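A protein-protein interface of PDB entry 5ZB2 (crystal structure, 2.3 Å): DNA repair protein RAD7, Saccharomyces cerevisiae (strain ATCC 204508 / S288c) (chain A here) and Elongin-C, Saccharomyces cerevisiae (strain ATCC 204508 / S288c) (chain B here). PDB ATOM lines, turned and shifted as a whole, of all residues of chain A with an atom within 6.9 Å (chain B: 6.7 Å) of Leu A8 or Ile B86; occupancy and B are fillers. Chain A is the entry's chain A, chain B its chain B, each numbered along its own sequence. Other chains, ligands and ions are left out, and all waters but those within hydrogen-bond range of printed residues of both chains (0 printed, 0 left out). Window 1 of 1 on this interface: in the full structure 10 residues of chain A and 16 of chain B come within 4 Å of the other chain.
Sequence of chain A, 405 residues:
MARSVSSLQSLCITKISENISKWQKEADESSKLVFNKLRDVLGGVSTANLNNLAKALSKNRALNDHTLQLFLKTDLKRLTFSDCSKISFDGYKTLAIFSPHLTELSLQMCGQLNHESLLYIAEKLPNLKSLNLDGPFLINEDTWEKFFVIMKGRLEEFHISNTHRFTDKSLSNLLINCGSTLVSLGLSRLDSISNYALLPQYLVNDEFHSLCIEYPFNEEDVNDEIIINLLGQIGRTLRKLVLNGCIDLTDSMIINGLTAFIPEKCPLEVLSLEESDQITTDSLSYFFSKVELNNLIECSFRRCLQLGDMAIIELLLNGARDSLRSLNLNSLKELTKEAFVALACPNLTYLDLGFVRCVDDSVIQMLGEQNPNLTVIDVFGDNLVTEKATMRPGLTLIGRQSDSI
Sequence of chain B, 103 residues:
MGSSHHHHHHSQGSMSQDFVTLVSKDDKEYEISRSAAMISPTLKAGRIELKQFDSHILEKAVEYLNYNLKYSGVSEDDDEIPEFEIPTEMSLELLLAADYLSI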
ATOM      1  N   VAL A   5     -16.678  29.012 -13.613  1.00  0.00           N
ATOM      2  CA  VAL A   5     -15.986  29.565 -14.771  1.00  0.00           C
ATOM      3  C   VAL A   5     -15.869  28.468 -15.820  1.00  0.00           C
ATOM      4  O   VAL A   5     -15.400  27.363 -15.520  1.00  0.00           O
ATOM      5  CB  VAL A   5     -14.598  30.111 -14.392  1.00  0.00           C
ATOM      6  CG1 VAL A   5     -13.854  30.608 -15.626  1.00  0.00           C
ATOM      7  CG2 VAL A   5     -14.733  31.223 -13.362  1.00  0.00           C
ATOM      8  N   SER A   6     -16.289  28.776 -17.046  1.00  0.00           N
ATOM      9  CA  SER A   6     -16.234  27.795 -18.122  1.00  0.00           C
ATOM     10  C   SER A   6     -14.791  27.416 -18.429  1.00  0.00           C
ATOM     11  O   SER A   6     -13.902  28.271 -18.487  1.00  0.00           O
ATOM     12  CB  SER A   6     -16.909  28.348 -19.378  1.00  0.00           C
ATOM     13  OG  SER A   6     -18.270  28.658 -19.132  1.00  0.00           O
ATOM     14  N   SER A   7     -14.562  26.120 -18.631  1.00  0.00           N
ATOM     15  CA  SER A   7     -13.229  25.635 -18.956  1.00  0.00           C
ATOM     16  C   SER A   7     -12.754  26.215 -20.283  1.00  0.00           C
ATOM     17  O   SER A   7     -13.552  26.559 -21.160  1.00  0.00           O
ATOM     18  CB  SER A   7     -13.223  24.109 -19.033  1.00  0.00           C
ATOM     19  OG  SER A   7     -13.988  23.663 -20.140  1.00  0.00           O
ATOM     20  N   LEU A   8     -11.432  26.310 -20.432  1.00  0.00           N
ATOM     21  CA  LEU A   8     -10.870  26.788 -21.691  1.00  0.00           C
ATOM     22  C   LEU A   8     -11.243  25.876 -22.852  1.00  0.00           C
ATOM     23  O   LEU A   8     -11.369  26.343 -23.991  1.00  0.00           O
ATOM     24  CB  LEU A   8      -9.350  26.903 -21.583  1.00  0.00           C
ATOM     25  CG  LEU A   8      -8.630  27.371 -22.852  1.00  0.00           C
ATOM     26  CD1 LEU A   8      -9.164  28.718 -23.334  1.00  0.00           C
ATOM     27  CD2 LEU A   8      -7.133  27.448 -22.607  1.00  0.00           C
ATOM     28  N   GLN A   9     -11.410  24.578 -22.593  1.00  0.00           N
ATOM     29  CA  GLN A   9     -11.842  23.662 -23.644  1.00  0.00           C
ATOM     30  C   GLN A   9     -13.229  24.037 -24.149  1.00  0.00           C
ATOM     31  O   GLN A   9     -13.462  24.126 -25.359  1.00  0.00           O
ATOM     32  CB  GLN A   9     -11.831  22.224 -23.123  1.00  0.00           C
ATOM     33  CG  GLN A   9     -10.467  21.729 -22.680  1.00  0.00           C
ATOM     34  CD  GLN A   9     -10.555  20.484 -21.815  1.00  0.00           C
ATOM     35  OE1 GLN A   9     -10.361  20.545 -20.600  1.00  0.00           O
ATOM     36  NE2 GLN A   9     -10.848  19.349 -22.437  1.00  0.00           N
ATOM     37  N   SER A  10     -14.164  24.264 -23.225  1.00  0.00           N
ATOM     38  CA  SER A  10     -15.516  24.646 -23.613  1.00  0.00           C
ATOM     39  C   SER A  10     -15.516  25.945 -24.407  1.00  0.00           C
ATOM     40  O   SER A  10     -16.262  26.084 -25.384  1.00  0.00           O
ATOM     41  CB  SER A  10     -16.395  24.780 -22.368  1.00  0.00           C
ATOM     42  OG  SER A  10     -17.702  25.194 -22.714  1.00  0.00           O
ATOM     43  N   LEU A  11     -14.677  26.907 -24.009  1.00  0.00           N
ATOM     44  CA  LEU A  11     -14.652  28.196 -24.693  1.00  0.00           C
ATOM     45  C   LEU A  11     -14.130  28.055 -26.116  1.00  0.00           C
ATOM     46  O   LEU A  11     -14.679  28.654 -27.047  1.00  0.00           O
ATOM     47  CB  LEU A  11     -13.800  29.193 -23.904  1.00  0.00           C
ATOM     48  CG  LEU A  11     -14.280  29.514 -22.488  1.00  0.00           C
ATOM     49  CD1 LEU A  11     -13.305  30.462 -21.808  1.00  0.00           C
ATOM     50  CD2 LEU A  11     -15.684  30.107 -22.499  1.00  0.00           C
ATOM     51  N   CYS A  12     -13.070  27.266 -26.307  1.00  0.00           N
ATOM     52  CA  CYS A  12     -12.583  27.013 -27.658  1.00  0.00           C
ATOM     53  C   CYS A  12     -13.643  26.313 -28.499  1.00  0.00           C
ATOM     54  O   CYS A  12     -13.800  26.610 -29.689  1.00  0.00           O
ATOM     55  CB  CYS A  12     -11.303  26.181 -27.610  1.00  0.00           C
ATOM     56  SG  CYS A  12      -9.869  27.038 -26.896  1.00  0.00           S
ATOM     57  N   ILE A  13     -14.385  25.380 -27.896  1.00  0.00           N
ATOM     58  CA  ILE A  13     -15.416  24.658 -28.637  1.00  0.00           C
ATOM     59  C   ILE A  13     -16.519  25.611 -29.078  1.00  0.00           C
ATOM     60  O   ILE A  13     -17.027  25.515 -30.200  1.00  0.00           O
ATOM     61  CB  ILE A  13     -15.959  23.493 -27.787  1.00  0.00           C
ATOM     62  CG1 ILE A  13     -14.886  22.401 -27.679  1.00  0.00           C
ATOM     63  CG2 ILE A  13     -17.252  22.930 -28.385  1.00  0.00           C
ATOM     64  CD1 ILE A  13     -15.227  21.275 -26.730  1.00  0.00           C
ATOM     65  N   LYS A  15     -16.149  28.831 -29.712  1.00  0.00           N
ATOM     66  CA  LYS A  15     -15.598  29.615 -30.811  1.00  0.00           C
ATOM     67  C   LYS A  15     -15.594  28.805 -32.100  1.00  0.00           C
ATOM     68  O   LYS A  15     -15.996  29.300 -33.160  1.00  0.00           O
ATOM     69  CB  LYS A  15     -14.185  30.089 -30.463  1.00  0.00           C
ATOM     70  CG  LYS A  15     -13.513  30.942 -31.543  1.00  0.00           C
ATOM     71  CD  LYS A  15     -14.367  32.135 -31.983  1.00  0.00           C
ATOM     72  CE  LYS A  15     -14.667  33.087 -30.832  1.00  0.00           C
ATOM     73  NZ  LYS A  15     -15.550  34.211 -31.253  1.00  0.00           N
ATOM     74  N   ASN A  19     -17.804  29.529 -35.590  1.00  0.00           N
ATOM     75  CA  ASN A  19     -17.198  29.768 -36.894  1.00  0.00           C
ATOM     76  C   ASN A  19     -17.612  28.729 -37.925  1.00  0.00           C
ATOM     77  O   ASN A  19     -17.604  29.023 -39.125  1.00  0.00           O
ATOM     78  CB  ASN A  19     -15.675  29.810 -36.772  1.00  0.00           C
ATOM     79  CG  ASN A  19     -15.168  31.177 -36.359  1.00  0.00           C
ATOM     80  OD1 ASN A  19     -14.987  32.061 -37.197  1.00  0.00           O
ATOM     81  ND2 ASN A  19     -14.944  31.361 -35.062  1.00  0.00           N
ATOM     82  N   LYS B  60      -1.630  32.627 -24.342  1.00  0.00           N
ATOM     83  CA  LYS B  60      -3.073  32.655 -24.139  1.00  0.00           C
ATOM     84  C   LYS B  60      -3.499  31.682 -23.046  1.00  0.00           C
ATOM     85  O   LYS B  60      -4.442  31.963 -22.297  1.00  0.00           O
ATOM     86  CB  LYS B  60      -3.799  32.337 -25.448  1.00  0.00           C
ATOM     87  CG  LYS B  60      -5.186  32.960 -25.559  1.00  0.00           C
ATOM     88  CD  LYS B  60      -5.110  34.481 -25.639  1.00  0.00           C
ATOM     89  CE  LYS B  60      -6.483  35.112 -25.756  1.00  0.00           C
ATOM     90  NZ  LYS B  60      -6.393  36.597 -25.849  1.00  0.00           N
ATOM     91  N   ALA B  61      -2.818  30.540 -22.940  1.00  0.00           N
ATOM     92  CA  ALA B  61      -3.103  29.607 -21.855  1.00  0.00           C
ATOM     93  C   ALA B  61      -2.861  30.262 -20.502  1.00  0.00           C
ATOM     94  O   ALA B  61      -3.715  30.209 -19.608  1.00  0.00           O
ATOM     95  CB  ALA B  61      -2.247  28.351 -22.008  1.00  0.00           C
ATOM     96  N   TYR B  64      -5.519  32.614 -19.685  1.00  0.00           N
ATOM     97  CA  TYR B  64      -6.725  31.985 -19.156  1.00  0.00           C
ATOM     98  C   TYR B  64      -6.545  31.578 -17.698  1.00  0.00           C
ATOM     99  O   TYR B  64      -7.455  31.762 -16.881  1.00  0.00           O
ATOM    100  CB  TYR B  64      -7.118  30.768 -19.995  1.00  0.00           C
ATOM    101  CG  TYR B  64      -8.245  29.982 -19.363  1.00  0.00           C
ATOM    102  CD1 TYR B  64      -9.567  30.360 -19.547  1.00  0.00           C
ATOM    103  CD2 TYR B  64      -7.985  28.881 -18.558  1.00  0.00           C
ATOM    104  CE1 TYR B  64     -10.602  29.658 -18.956  1.00  0.00           C
ATOM    105  CE2 TYR B  64      -9.012  28.173 -17.963  1.00  0.00           C
ATOM    106  CZ  TYR B  64     -10.319  28.565 -18.166  1.00  0.00           C
ATOM    107  OH  TYR B  64     -11.347  27.865 -17.576  1.00  0.00           O
ATOM    108  N   LEU B  65      -5.386  31.009 -17.354  1.00  0.00           N
ATOM    109  CA  LEU B  65      -5.155  30.574 -15.980  1.00  0.00           C
ATOM    110  C   LEU B  65      -5.338  31.729 -15.006  1.00  0.00           C
ATOM    111  O   LEU B  65      -6.096  31.625 -14.035  1.00  0.00           O
ATOM    112  CB  LEU B  65      -3.755  29.972 -15.848  1.00  0.00           C
ATOM    113  CG  LEU B  65      -3.513  28.654 -16.584  1.00  0.00           C
ATOM    114  CD1 LEU B  65      -2.052  28.252 -16.481  1.00  0.00           C
ATOM    115  CD2 LEU B  65      -4.405  27.547 -16.038  1.00  0.00           C
ATOM    116  N   ASN B  68      -8.780  32.614 -14.852  1.00  0.00           N
ATOM    117  CA  ASN B  68      -9.579  31.645 -14.110  1.00  0.00           C
ATOM    118  C   ASN B  68      -9.501  31.904 -12.611  1.00  0.00           C
ATOM    119  O   ASN B  68     -10.530  32.018 -11.936  1.00  0.00           O
ATOM    120  CB  ASN B  68      -9.119  30.224 -14.435  1.00  0.00           C
ATOM    121  CG  ASN B  68     -10.011  29.166 -13.813  1.00  0.00           C
ATOM    122  OD1 ASN B  68      -9.979  28.942 -12.603  1.00  0.00           O
ATOM    123  ND2 ASN B  68     -10.812  28.508 -14.641  1.00  0.00           N
ATOM    124  N   PHE B  84     -13.755  35.512 -21.957  1.00  0.00           N
ATOM    125  CA  PHE B  84     -12.370  35.291 -22.357  1.00  0.00           C
ATOM    126  C   PHE B  84     -12.321  35.227 -23.878  1.00  0.00           C
ATOM    127  O   PHE B  84     -12.824  34.275 -24.483  1.00  0.00           O
ATOM    128  CB  PHE B  84     -11.824  34.013 -21.728  1.00  0.00           C
ATOM    129  CG  PHE B  84     -10.373  33.773 -22.012  1.00  0.00           C
ATOM    130  CD1 PHE B  84      -9.398  34.291 -21.179  1.00  0.00           C
ATOM    131  CD2 PHE B  84      -9.981  33.028 -23.112  1.00  0.00           C
ATOM    132  CE1 PHE B  84      -8.060  34.075 -21.437  1.00  0.00           C
ATOM    133  CE2 PHE B  84      -8.644  32.806 -23.374  1.00  0.00           C
ATOM    134  CZ  PHE B  84      -7.681  33.331 -22.535  1.00  0.00           C
ATOM    135  N   GLU B  85     -11.727  36.243 -24.496  1.00  0.00           N
ATOM    136  CA  GLU B  85     -11.630  36.284 -25.947  1.00  0.00           C
ATOM    137  C   GLU B  85     -10.665  35.217 -26.449  1.00  0.00           C
ATOM    138  O   GLU B  85      -9.595  34.999 -25.873  1.00  0.00           O
ATOM    139  CB  GLU B  85     -11.172  37.667 -26.406  1.00  0.00           C
ATOM    140  CG  GLU B  85     -12.130  38.789 -26.038  1.00  0.00           C
ATOM    141  CD  GLU B  85     -11.599  40.160 -26.415  1.00  0.00           C
ATOM    142  OE1 GLU B  85     -10.395  40.266 -26.735  1.00  0.00           O
ATOM    143  OE2 GLU B  85     -12.383  41.131 -26.392  1.00  0.00           O
ATOM    144  N   ILE B  86     -11.052  34.547 -27.531  1.00  0.00           N
ATOM    145  CA  ILE B  86     -10.227  33.509 -28.143  1.00  0.00           C
ATOM    146  C   ILE B  86     -10.107  33.811 -29.632  1.00  0.00           C
ATOM    147  O   ILE B  86     -11.111  33.737 -30.355  1.00  0.00           O
ATOM    148  CB  ILE B  86     -10.818  32.111 -27.900  1.00  0.00           C
ATOM    149  CG1 ILE B  86     -10.747  31.767 -26.409  1.00  0.00           C
ATOM    150  CG2 ILE B  86     -10.080  31.062 -28.732  1.00  0.00           C
ATOM    151  CD1 ILE B  86     -11.390  30.446 -26.030  1.00  0.00           C
ATOM    152  N   PRO B  87      -8.919  34.145 -30.140  1.00  0.00           N
ATOM    153  CA  PRO B  87      -8.799  34.440 -31.574  1.00  0.00           C
ATOM    154  C   PRO B  87      -9.209  33.247 -32.422  1.00  0.00           C
ATOM    155  O   PRO B  87      -8.863  32.102 -32.125  1.00  0.00           O
ATOM    156  CB  PRO B  87      -7.312  34.773 -31.750  1.00  0.00           C
ATOM    157  CG  PRO B  87      -6.811  35.098 -30.389  1.00  0.00           C
ATOM    158  CD  PRO B  87      -7.632  34.292 -29.438  1.00  0.00           C
ATOM    159  N   THR B  88      -9.955  33.529 -33.494  1.00  0.00           N
ATOM    160  CA  THR B  88     -10.415  32.463 -34.380  1.00  0.00           C
ATOM    161  C   THR B  88      -9.241  31.688 -34.968  1.00  0.00           C
ATOM    162  O   THR B  88      -9.282  30.455 -35.057  1.00  0.00           O
ATOM    163  CB  THR B  88     -11.279  33.052 -35.497  1.00  0.00           C
ATOM    164  OG1 THR B  88     -12.425  33.697 -34.926  1.00  0.00           O
ATOM    165  CG2 THR B  88     -11.742  31.968 -36.467  1.00  0.00           C
ATOM    166  N   GLU B  89      -8.184  32.393 -35.370  1.00  0.00           N
ATOM    167  CA  GLU B  89      -7.048  31.776 -36.047  1.00  0.00           C
ATOM    168  C   GLU B  89      -6.263  30.805 -35.168  1.00  0.00           C
ATOM    169  O   GLU B  89      -5.319  30.182 -35.665  1.00  0.00           O
ATOM    170  CB  GLU B  89      -6.102  32.861 -36.567  1.00  0.00           C
ATOM    171  CG  GLU B  89      -5.577  33.793 -35.484  1.00  0.00           C
ATOM    172  CD  GLU B  89      -6.183  35.181 -35.562  1.00  0.00           C
ATOM    173  OE1 GLU B  89      -5.443  36.131 -35.895  1.00  0.00           O
ATOM    174  OE2 GLU B  89      -7.395  35.321 -35.297  1.00  0.00           O
ATOM    175  N   MET B  90      -6.609  30.656 -33.888  1.00  0.00           N
ATOM    176  CA  MET B  90      -5.914  29.722 -33.007  1.00  0.00           C
ATOM    177  C   MET B  90      -6.887  28.893 -32.174  1.00  0.00           C
ATOM    178  O   MET B  90      -6.496  28.343 -31.137  1.00  0.00           O
ATOM    179  CB  MET B  90      -4.947  30.473 -32.087  1.00  0.00           C
ATOM    180  CG  MET B  90      -5.634  31.381 -31.076  1.00  0.00           C
ATOM    181  SD  MET B  90      -4.478  32.238 -29.985  1.00  0.00           S
ATOM    182  CE  MET B  90      -3.540  33.212 -31.161  1.00  0.00           C
ATOM    183  N   SER B  91      -8.145  28.785 -32.607  1.00  0.00           N
ATOM    184  CA  SER B  91      -9.142  28.077 -31.810  1.00  0.00           C
ATOM    185  C   SER B  91      -8.851  26.580 -31.753  1.00  0.00           C
ATOM    186  O   SER B  91      -8.972  25.961 -30.690  1.00  0.00           O
ATOM    187  CB  SER B  91     -10.542  28.336 -32.365  1.00  0.00           C
ATOM    188  OG  SER B  91     -10.614  28.030 -33.746  1.00  0.00           O
ATOM    189  N   LEU B  94      -5.509  25.912 -29.752  1.00  0.00           N
ATOM    190  CA  LEU B  94      -5.731  26.226 -28.345  1.00  0.00           C
ATOM    191  C   LEU B  94      -6.601  25.173 -27.668  1.00  0.00           C
ATOM    192  O   LEU B  94      -6.405  24.882 -26.482  1.00  0.00           O
ATOM    193  CB  LEU B  94      -6.364  27.611 -28.201  1.00  0.00           C
ATOM    194  CG  LEU B  94      -6.527  28.131 -26.768  1.00  0.00           C
ATOM    195  CD1 LEU B  94      -5.187  28.190 -26.045  1.00  0.00           C
ATOM    196  CD2 LEU B  94      -7.190  29.503 -26.759  1.00  0.00           C
ATOM    197  N   LEU B  95      -7.561  24.594 -28.392  1.00  0.00           N
ATOM    198  CA  LEU B  95      -8.357  23.510 -27.826  1.00  0.00           C
ATOM    199  C   LEU B  95      -7.468  22.335 -27.437  1.00  0.00           C
ATOM    200  O   LEU B  95      -7.607  21.771 -26.345  1.00  0.00           O
ATOM    201  CB  LEU B  95      -9.432  23.065 -28.820  1.00  0.00           C
ATOM    202  CG  LEU B  95     -10.200  21.790 -28.451  1.00  0.00           C
ATOM    203  CD1 LEU B  95     -10.847  21.909 -27.075  1.00  0.00           C
ATOM    204  CD2 LEU B  95     -11.249  21.493 -29.505  1.00  0.00           C
ATOM    205  N   ALA B  97      -4.333  22.378 -26.648  1.00  0.00           N
ATOM    206  CA  ALA B  97      -3.526  22.724 -25.482  1.00  0.00           C
ATOM    207  C   ALA B  97      -4.355  22.673 -24.205  1.00  0.00           C
ATOM    208  O   ALA B  97      -3.881  22.191 -23.170  1.00  0.00           O
ATOM    209  CB  ALA B  97      -2.904  24.106 -25.663  1.00  0.00           C
ATOM    210  N   ALA B  98      -5.593  23.167 -24.257  1.00  0.00           N
ATOM    211  CA  ALA B  98      -6.458  23.108 -23.085  1.00  0.00           C
ATOM    212  C   ALA B  98      -6.741  21.665 -22.691  1.00  0.00           C
ATOM    213  O   ALA B  98      -6.832  21.344 -21.500  1.00  0.00           O
ATOM    214  CB  ALA B  98      -7.766  23.852 -23.355  1.00  0.00           C
ATOM    215  N   LEU B 101      -3.625  20.221 -21.023  1.00  0.00           N
ATOM    216  CA  LEU B 101      -3.548  20.831 -19.703  1.00  0.00           C
ATOM    217  C   LEU B 101      -4.774  20.551 -18.847  1.00  0.00           C
ATOM    218  O   LEU B 101      -4.757  20.865 -17.652  1.00  0.00           O
ATOM    219  CB  LEU B 101      -3.361  22.345 -19.836  1.00  0.00           C
ATOM    220  CG  LEU B 101      -2.095  22.812 -20.554  1.00  0.00           C
ATOM    221  CD1 LEU B 101      -2.100  24.324 -20.686  1.00  0.00           C
ATOM    222  CD2 LEU B 101      -0.844  22.342 -19.825  1.00  0.00           C
ATOM    223  N   ILE B 103      -7.584  22.043 -18.763  1.00  0.00           N
ATOM    224  CA  ILE B 103      -8.118  23.312 -18.284  1.00  0.00           C
ATOM    225  C   ILE B 103      -9.290  23.750 -19.151  1.00  0.00           C
ATOM    226  O   ILE B 103      -9.970  24.727 -18.834  1.00  0.00           O
ATOM    227  CB  ILE B 103      -7.028  24.394 -18.258  1.00  0.00           C
ATOM    228  CG1 ILE B 103      -6.413  24.560 -19.652  1.00  0.00           C
ATOM    229  CG2 ILE B 103      -5.969  24.036 -17.221  1.00  0.00           C
ATOM    230  CD1 ILE B 103      -5.381  25.664 -19.750  1.00  0.00           C
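The side-chain hydroxyl of Tyr B64 sits at hydrogen-bond distance from the backbone carbonyl oxygen of Ser A6 (2.7 Å). The backbone NH (N) of Leu A8 is in hydrogen-bond range of the side-chain hydroxyl (OH) of Tyr B64 (3.3 Å). The backbone NH (N) of Leu A8 sits at hydrogen-bond distance from the backbone carbonyl oxygen (O) of Ile B103. The side-chain sulfur (SG) of Cys A12 lies within hydrogen-bond range of the backbone NH (N) of Leu B95, at 3.7 Å. The side-chain amide nitrogen (ND2) of Asn A19 is in hydrogen-bond range of the side-chain hydroxyl (OG1) of Thr B88 (3.4 Å).
The side-chain hydroxyl (OG) of Ser A7 lies within hydrogen-bond range of the backbone NH (N) of Ser A10, at 3.1 Å. O of Leu A8 sits at hydrogen-bond distance from SG of Cys A12 (3.3 Å). The backbone carbonyl oxygen of Lys A15 lies within hydrogen-bond range of the side-chain amide nitrogen of Asn A19. OH of Tyr B64 lies within hydrogen-bond range of ND2 of Asn B68, 3.1 Å away. O of Thr B88 is in hydrogen-bond range of OG of Ser B91, at 3.1 Å. The backbone carbonyl oxygen (O) of Ala B98 is in hydrogen-bond range of the backbone NH (N) of Ile B103 (2.9 Å).
Asn B68 touches Val A5. OH of Tyr B64 touches CA of Ser A7, at 3.2 Å. CB of Ser A7 touches O of Ile B103, 3.3 Å away. Leu A8 touches Ile B86 (CD1 to CD1, 3.9 Å). Leu B95 touches Gln A9 (CD1 to O, 3.8 Å). CB of Ala B98 touches CG of Gln A9 (3.5 Å). N of Ile B103 touches OE1 of Gln A9, 3.7 Å away. CD1 of Leu A11 touches CB of Phe B84, 3.8 Å away. Cys A12 touches Ile B86. Lys A15 touches Ile B86 (CE to O, 3.6 Å).
Of the printed residues of chain B, Leu A8 touches Tyr B64 (3.3 Å), Ile B86 (3.9 Å), Ala B98 (3.7 Å) and Ile B103 (2.7 Å). Of chain A, only Leu A8 (3.9 Å), Leu A11 (3.4 Å), Cys A12 (3.6 Å) and Lys A15 (3.6 Å) come within 4 Å of Ile B86. Of the printed residues of chain A, Leu B95 touches Gln A9 (3.8 Å) and Cys A12 (3.7 Å). Of the printed residues of chain A, Leu B94 touches Cys A12 (3.5 Å). Of the printed residues of chain B, Leu A11 touches Phe B84 and Ile B86. The nearest printed residue of chain B that does not touch Leu A8 is Leu B94 (4.02 Å).
Printed residues of chain A that touch a printed residue of chain B: Val A5, Ser A6, Ser A7, Leu A8, Gln A9, Leu A11, Cys A12, Lys A15 and Asn A19. Among the printed residues, 20 pairs touch across the chains.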
